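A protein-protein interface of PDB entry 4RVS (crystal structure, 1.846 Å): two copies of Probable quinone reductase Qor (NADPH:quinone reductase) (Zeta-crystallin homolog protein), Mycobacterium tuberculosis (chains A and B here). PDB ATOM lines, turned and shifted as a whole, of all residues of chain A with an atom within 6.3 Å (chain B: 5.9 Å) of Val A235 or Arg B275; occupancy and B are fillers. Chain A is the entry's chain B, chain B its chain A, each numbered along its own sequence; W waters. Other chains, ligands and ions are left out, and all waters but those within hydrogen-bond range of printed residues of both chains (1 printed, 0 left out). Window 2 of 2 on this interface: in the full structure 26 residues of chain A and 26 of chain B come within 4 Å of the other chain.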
ATOM      1  N   ARG A 206      15.653 -22.874 -38.421  1.00  0.00           N
ATOM      2  CA  ARG A 206      16.330 -22.731 -37.139  1.00  0.00           C
ATOM      3  C   ARG A 206      17.855 -22.799 -37.288  1.00  0.00           C
ATOM      4  O   ARG A 206      18.578 -22.072 -36.608  1.00  0.00           O
ATOM      5  CB  ARG A 206      15.786 -23.724 -36.102  1.00  0.00           C
ATOM      6  CG  ARG A 206      14.372 -23.353 -35.649  1.00  0.00           C
ATOM      7  CD  ARG A 206      13.808 -24.224 -34.529  1.00  0.00           C
ATOM      8  NE  ARG A 206      12.370 -23.993 -34.414  1.00  0.00           N
ATOM      9  CZ  ARG A 206      11.825 -22.925 -33.827  1.00  0.00           C
ATOM     10  NH1 ARG A 206      12.592 -21.991 -33.279  1.00  0.00           N
ATOM     11  NH2 ARG A 206      10.505 -22.783 -33.792  1.00  0.00           N
ATOM     12  N   THR A 212      17.300 -20.068 -33.166  1.00  0.00           N
ATOM     13  CA  THR A 212      16.284 -19.188 -32.593  1.00  0.00           C
ATOM     14  C   THR A 212      14.928 -19.288 -33.290  1.00  0.00           C
ATOM     15  O   THR A 212      13.886 -19.286 -32.636  1.00  0.00           O
ATOM     16  CB  THR A 212      16.760 -17.721 -32.603  1.00  0.00           C
ATOM     17  OG1 THR A 212      17.951 -17.605 -31.812  1.00  0.00           O
ATOM     18  CG2 THR A 212      15.689 -16.785 -32.032  1.00  0.00           C
ATOM     19  N   VAL A 214      12.546 -17.464 -36.537  1.00  0.00           N
ATOM     20  CA  VAL A 214      12.336 -16.092 -37.006  1.00  0.00           C
ATOM     21  C   VAL A 214      11.393 -15.327 -36.088  1.00  0.00           C
ATOM     22  O   VAL A 214      10.475 -15.916 -35.485  1.00  0.00           O
ATOM     23  CB  VAL A 214      11.801 -16.032 -38.474  1.00  0.00           C
ATOM     24  CG1 VAL A 214      12.847 -16.532 -39.467  1.00  0.00           C
ATOM     25  CG2 VAL A 214      10.515 -16.828 -38.622  1.00  0.00           C
ATOM     26  N   LEU A 233       8.893 -20.342 -35.979  1.00  0.00           N
ATOM     27  CA  LEU A 233       8.873 -19.100 -35.211  1.00  0.00           C
ATOM     28  C   LEU A 233       9.754 -19.096 -33.964  1.00  0.00           C
ATOM     29  O   LEU A 233       9.861 -20.093 -33.245  1.00  0.00           O
ATOM     30  CB  LEU A 233       7.435 -18.770 -34.804  1.00  0.00           C
ATOM     31  CG  LEU A 233       6.559 -18.215 -35.920  1.00  0.00           C
ATOM     32  CD1 LEU A 233       5.098 -18.363 -35.532  1.00  0.00           C
ATOM     33  CD2 LEU A 233       6.900 -16.744 -36.180  1.00  0.00           C
ATOM     34  N   ALA A 234      10.382 -17.953 -33.705  1.00  0.00           N
ATOM     35  CA  ALA A 234      11.057 -17.733 -32.425  1.00  0.00           C
ATOM     36  C   ALA A 234      10.010 -17.665 -31.311  1.00  0.00           C
ATOM     37  O   ALA A 234       8.834 -17.403 -31.572  1.00  0.00           O
ATOM     38  CB  ALA A 234      11.879 -16.452 -32.472  1.00  0.00           C
ATOM     39  N   VAL A 235      10.428 -17.909 -30.071  1.00  0.00           N
ATOM     40  CA  VAL A 235       9.517 -17.783 -28.928  1.00  0.00           C
ATOM     41  C   VAL A 235       8.838 -16.414 -28.948  1.00  0.00           C
ATOM     42  O   VAL A 235       9.501 -15.395 -29.159  1.00  0.00           O
ATOM     43  CB  VAL A 235      10.258 -17.987 -27.594  1.00  0.00           C
ATOM     44  CG1 VAL A 235       9.377 -17.588 -26.397  1.00  0.00           C
ATOM     45  CG2 VAL A 235      10.701 -19.439 -27.461  1.00  0.00           C
ATOM     46  N   ARG A 236       7.518 -16.419 -28.760  1.00  0.00           N
ATOM     47  CA  ARG A 236       6.672 -15.216 -28.806  1.00  0.00           C
ATOM     48  C   ARG A 236       6.683 -14.481 -30.150  1.00  0.00           C
ATOM     49  O   ARG A 236       6.317 -13.300 -30.222  1.00  0.00           O
ATOM     50  CB  ARG A 236       7.002 -14.256 -27.652  1.00  0.00           C
ATOM     51  CG  ARG A 236       6.656 -14.822 -26.263  1.00  0.00           C
ATOM     52  CD  ARG A 236       7.368 -14.018 -25.166  1.00  0.00           C
ATOM     53  NE  ARG A 236       6.967 -12.613 -25.208  1.00  0.00           N
ATOM     54  CZ  ARG A 236       7.526 -11.630 -24.506  1.00  0.00           C
ATOM     55  NH1 ARG A 236       8.529 -11.875 -23.675  1.00  0.00           N
ATOM     56  NH2 ARG A 236       7.069 -10.388 -24.643  1.00  0.00           N
ATOM     57  N   GLY A 237       7.057 -15.187 -31.214  1.00  0.00           N
ATOM     58  CA  GLY A 237       7.041 -14.609 -32.551  1.00  0.00           C
ATOM     59  C   GLY A 237       5.629 -14.437 -33.097  1.00  0.00           C
ATOM     60  O   GLY A 237       4.663 -14.904 -32.486  1.00  0.00           O
ATOM     61  N   ALA A 260       4.363 -24.072 -30.222  1.00  0.00           N
ATOM     62  CA  ALA A 260       5.245 -23.369 -31.148  1.00  0.00           C
ATOM     63  C   ALA A 260       6.100 -22.295 -30.471  1.00  0.00           C
ATOM     64  O   ALA A 260       7.033 -21.760 -31.091  1.00  0.00           O
ATOM     65  CB  ALA A 260       4.438 -22.764 -32.295  1.00  0.00           C
ATOM     66  N   GLY A 261       5.772 -21.976 -29.215  1.00  0.00           N
ATOM     67  CA  GLY A 261       6.543 -21.028 -28.426  1.00  0.00           C
ATOM     68  C   GLY A 261       5.760 -19.836 -27.906  1.00  0.00           C
ATOM     69  O   GLY A 261       6.296 -18.725 -27.879  1.00  0.00           O
ATOM     70  N   SER A 262       4.516 -20.065 -27.472  1.00  0.00           N
ATOM     71  CA  SER A 262       3.619 -18.984 -27.054  1.00  0.00           C
ATOM     72  C   SER A 262       3.572 -17.887 -28.126  1.00  0.00           C
ATOM     73  O   SER A 262       3.772 -16.708 -27.835  1.00  0.00           O
ATOM     74  CB  SER A 262       4.042 -18.413 -25.696  1.00  0.00           C
ATOM     75  OG  SER A 262       3.837 -19.378 -24.674  1.00  0.00           O
ATOM     76  N   VAL A 263       3.315 -18.292 -29.363  1.00  0.00           N
ATOM     77  CA  VAL A 263       3.384 -17.365 -30.486  1.00  0.00           C
ATOM     78  C   VAL A 263       2.060 -16.651 -30.680  1.00  0.00           C
ATOM     79  O   VAL A 263       1.060 -16.980 -30.041  1.00  0.00           O
ATOM     80  CB  VAL A 263       3.771 -18.093 -31.793  1.00  0.00           C
ATOM     81  CG1 VAL A 263       5.072 -18.866 -31.599  1.00  0.00           C
ATOM     82  CG2 VAL A 263       2.656 -19.037 -32.240  1.00  0.00           C
ATOM     83  N   LEU B 270       3.462 -19.904 -18.914  1.00  0.00           N
ATOM     84  CA  LEU B 270       4.462 -19.215 -18.098  1.00  0.00           C
ATOM     85  C   LEU B 270       5.911 -19.552 -18.448  1.00  0.00           C
ATOM     86  O   LEU B 270       6.801 -18.699 -18.347  1.00  0.00           O
ATOM     87  CB  LEU B 270       4.194 -19.516 -16.624  1.00  0.00           C
ATOM     88  CG  LEU B 270       5.134 -18.852 -15.633  1.00  0.00           C
ATOM     89  CD1 LEU B 270       5.018 -17.342 -15.724  1.00  0.00           C
ATOM     90  CD2 LEU B 270       4.795 -19.335 -14.233  1.00  0.00           C
ATOM     91  N   PHE B 271       6.139 -20.795 -18.862  1.00  0.00           N
ATOM     92  CA  PHE B 271       7.462 -21.265 -19.251  1.00  0.00           C
ATOM     93  C   PHE B 271       8.174 -20.305 -20.203  1.00  0.00           C
ATOM     94  O   PHE B 271       9.369 -20.063 -20.066  1.00  0.00           O
ATOM     95  CB  PHE B 271       7.335 -22.649 -19.901  1.00  0.00           C
ATOM     96  CG  PHE B 271       8.629 -23.219 -20.401  1.00  0.00           C
ATOM     97  CD1 PHE B 271       9.526 -23.813 -19.526  1.00  0.00           C
ATOM     98  CD2 PHE B 271       8.931 -23.196 -21.758  1.00  0.00           C
ATOM     99  CE1 PHE B 271      10.715 -24.356 -19.990  1.00  0.00           C
ATOM    100  CE2 PHE B 271      10.117 -23.738 -22.232  1.00  0.00           C
ATOM    101  CZ  PHE B 271      11.011 -24.321 -21.344  1.00  0.00           C
ATOM    102  N   HIS B 272       7.435 -19.747 -21.157  1.00  0.00           N
ATOM    103  CA  HIS B 272       8.048 -18.905 -22.183  1.00  0.00           C
ATOM    104  C   HIS B 272       8.245 -17.463 -21.725  1.00  0.00           C
ATOM    105  O   HIS B 272       8.731 -16.625 -22.488  1.00  0.00           O
ATOM    106  CB  HIS B 272       7.230 -18.962 -23.479  1.00  0.00           C
ATOM    107  CG  HIS B 272       7.261 -20.300 -24.149  1.00  0.00           C
ATOM    108  ND1 HIS B 272       6.118 -20.989 -24.490  1.00  0.00           N
ATOM    109  CD2 HIS B 272       8.300 -21.081 -24.537  1.00  0.00           C
ATOM    110  CE1 HIS B 272       6.448 -22.135 -25.060  1.00  0.00           C
ATOM    111  NE2 HIS B 272       7.766 -22.216 -25.104  1.00  0.00           N
ATOM    112  N   PHE B 273       7.885 -17.184 -20.475  1.00  0.00           N
ATOM    113  CA  PHE B 273       8.043 -15.844 -19.917  1.00  0.00           C
ATOM    114  C   PHE B 273       8.889 -15.868 -18.640  1.00  0.00           C
ATOM    115  O   PHE B 273       8.937 -14.888 -17.898  1.00  0.00           O
ATOM    116  CB  PHE B 273       6.668 -15.203 -19.657  1.00  0.00           C
ATOM    117  CG  PHE B 273       5.804 -15.114 -20.885  1.00  0.00           C
ATOM    118  CD1 PHE B 273       5.694 -13.919 -21.586  1.00  0.00           C
ATOM    119  CD2 PHE B 273       5.135 -16.239 -21.367  1.00  0.00           C
ATOM    120  CE1 PHE B 273       4.908 -13.838 -22.730  1.00  0.00           C
ATOM    121  CE2 PHE B 273       4.350 -16.171 -22.516  1.00  0.00           C
ATOM    122  CZ  PHE B 273       4.241 -14.973 -23.201  1.00  0.00           C
ATOM    123  N   THR B 274       9.559 -16.989 -18.395  1.00  0.00           N
ATOM    124  CA  THR B 274      10.456 -17.118 -17.253  1.00  0.00           C
ATOM    125  C   THR B 274      11.743 -17.792 -17.725  1.00  0.00           C
ATOM    126  O   THR B 274      12.275 -18.664 -17.055  1.00  0.00           O
ATOM    127  CB  THR B 274       9.818 -17.934 -16.091  1.00  0.00           C
ATOM    128  OG1 THR B 274       9.337 -19.199 -16.575  1.00  0.00           O
ATOM    129  CG2 THR B 274       8.666 -17.170 -15.461  1.00  0.00           C
ATOM    130  N   ARG B 275      12.239 -17.357 -18.882  1.00  0.00           N
ATOM    131  CA  ARG B 275      13.285 -18.082 -19.604  1.00  0.00           C
ATOM    132  C   ARG B 275      14.684 -17.933 -19.012  1.00  0.00           C
ATOM    133  O   ARG B 275      15.559 -18.771 -19.255  1.00  0.00           O
ATOM    134  CB  ARG B 275      13.303 -17.638 -21.072  1.00  0.00           C
ATOM    135  CG  ARG B 275      11.933 -17.688 -21.753  1.00  0.00           C
ATOM    136  CD  ARG B 275      12.017 -17.282 -23.225  1.00  0.00           C
ATOM    137  NE  ARG B 275      12.783 -18.255 -23.996  1.00  0.00           N
ATOM    138  CZ  ARG B 275      13.351 -18.001 -25.170  1.00  0.00           C
ATOM    139  NH1 ARG B 275      13.241 -16.798 -25.714  1.00  0.00           N
ATOM    140  NH2 ARG B 275      14.031 -18.949 -25.795  1.00  0.00           N
ATOM    141  N   THR B 276      14.906 -16.851 -18.272  1.00  0.00           N
ATOM    142  CA  THR B 276      16.180 -16.597 -17.614  1.00  0.00           C
ATOM    143  C   THR B 276      15.886 -16.083 -16.216  1.00  0.00           C
ATOM    144  O   THR B 276      14.765 -15.647 -15.939  1.00  0.00           O
ATOM    145  CB  THR B 276      16.993 -15.515 -18.349  1.00  0.00           C
ATOM    146  OG1 THR B 276      16.237 -14.297 -18.378  1.00  0.00           O
ATOM    147  CG2 THR B 276      17.308 -15.935 -19.775  1.00  0.00           C
ATOM    148  N   GLY B 277      16.885 -16.130 -15.338  1.00  0.00           N
ATOM    149  CA  GLY B 277      16.724 -15.612 -13.990  1.00  0.00           C
ATOM    150  C   GLY B 277      16.465 -14.122 -14.019  1.00  0.00           C
ATOM    151  O   GLY B 277      15.730 -13.588 -13.180  1.00  0.00           O
ATOM    152  N   GLU B 279      14.785 -12.433 -16.347  1.00  0.00           N
ATOM    153  CA  GLU B 279      13.376 -12.217 -16.679  1.00  0.00           C
ATOM    154  C   GLU B 279      12.485 -12.584 -15.486  1.00  0.00           C
ATOM    155  O   GLU B 279      11.565 -11.846 -15.135  1.00  0.00           O
ATOM    156  CB  GLU B 279      12.976 -13.034 -17.912  1.00  0.00           C
ATOM    157  CG  GLU B 279      11.550 -12.743 -18.379  1.00  0.00           C
ATOM    158  CD  GLU B 279      11.158 -13.521 -19.619  1.00  0.00           C
ATOM    159  OE1 GLU B 279      11.741 -14.606 -19.876  1.00  0.00           O
ATOM    160  OE2 GLU B 279      10.254 -13.043 -20.340  1.00  0.00           O
ATOM    161  N   PHE B 280      12.773 -13.720 -14.861  1.00  0.00           N
ATOM    162  CA  PHE B 280      12.015 -14.156 -13.693  1.00  0.00           C
ATOM    163  C   PHE B 280      12.057 -13.097 -12.595  1.00  0.00           C
ATOM    164  O   PHE B 280      11.030 -12.732 -12.026  1.00  0.00           O
ATOM    165  CB  PHE B 280      12.577 -15.471 -13.162  1.00  0.00           C
ATOM    166  CG  PHE B 280      11.752 -16.081 -12.059  1.00  0.00           C
ATOM    167  CD1 PHE B 280      10.738 -16.975 -12.356  1.00  0.00           C
ATOM    168  CD2 PHE B 280      11.995 -15.761 -10.725  1.00  0.00           C
ATOM    169  CE1 PHE B 280       9.974 -17.554 -11.339  1.00  0.00           C
ATOM    170  CE2 PHE B 280      11.238 -16.325  -9.711  1.00  0.00           C
ATOM    171  CZ  PHE B 280      10.224 -17.217 -10.020  1.00  0.00           C
HETATM  172  O   HOH W   1       9.758 -14.178 -22.666  1.00  0.00           O
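Val A235 touches two residues of chain B. Arg B275 touches one residue of chain A. Printed residues of chain B within 4 Å of Arg A236: His B272, Phe B273 and Glu B279. Of the printed residues of chain A, Glu B279 touches Arg A236. Of the printed residues of chain B, Gly A261 touches His B272 (3.5 Å). Of the printed residues of chain A, His B272 touches Val A235, Arg A236, Gly A261 and Ser A262. Of the printed residues of chain A, Phe B273 touches Arg A236 and Ser A262. Leu A233 touches none of the printed residues of chain B. Arg A206 touches none of the printed residues of chain B. The nearest printed residue of chain B that does not touch Arg A236 is Arg B275 (6.0 Å).
Water W1 lies within hydrogen-bond range of the side-chain carboxylate (OE2) of Glu B279 (2.6 Å), the backbone carbonyl oxygen (O) of His B272 (2.7 Å) and the guanidinium group (NH1) of Arg A236 (2.8 Å).
The side-chain hydroxyl (OG) of Ser A262 lies within hydrogen-bond range of a ring nitrogen (ND1) of His B272. The guanidinium group of Arg A236 lies within salt-bridge range of the side-chain carboxylate of Glu B279 (3.9 Å).
No position is printed for both chains.
Of the 10 printed residues of chain B, 4 touch a printed residue of chain A. Of the 12 printed residues of chain A, 4 touch a printed residue of chain B. Among the printed residues, 8 pairs touch across the chains.
Among the printed residues, merely in contact across the chains: Arg A236 with Phe B273, Gly A261 with His B272, Val A235 with Arg B275, Val A235 with His B272, Ser A262 with Phe B273 and Arg A236 with His B272.
The backbone NH of Arg B275 is in hydrogen-bond range of the side-chain carboxylate of Glu B279, at 3.0 Å. The side-chain hydroxyl (OG1) of Thr B276 lies within hydrogen-bond range of the backbone NH (N) of Glu B279 (3.1 Å). O of Gly A261 sits at hydrogen-bond distance from N of Arg A236 (2.8 Å).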
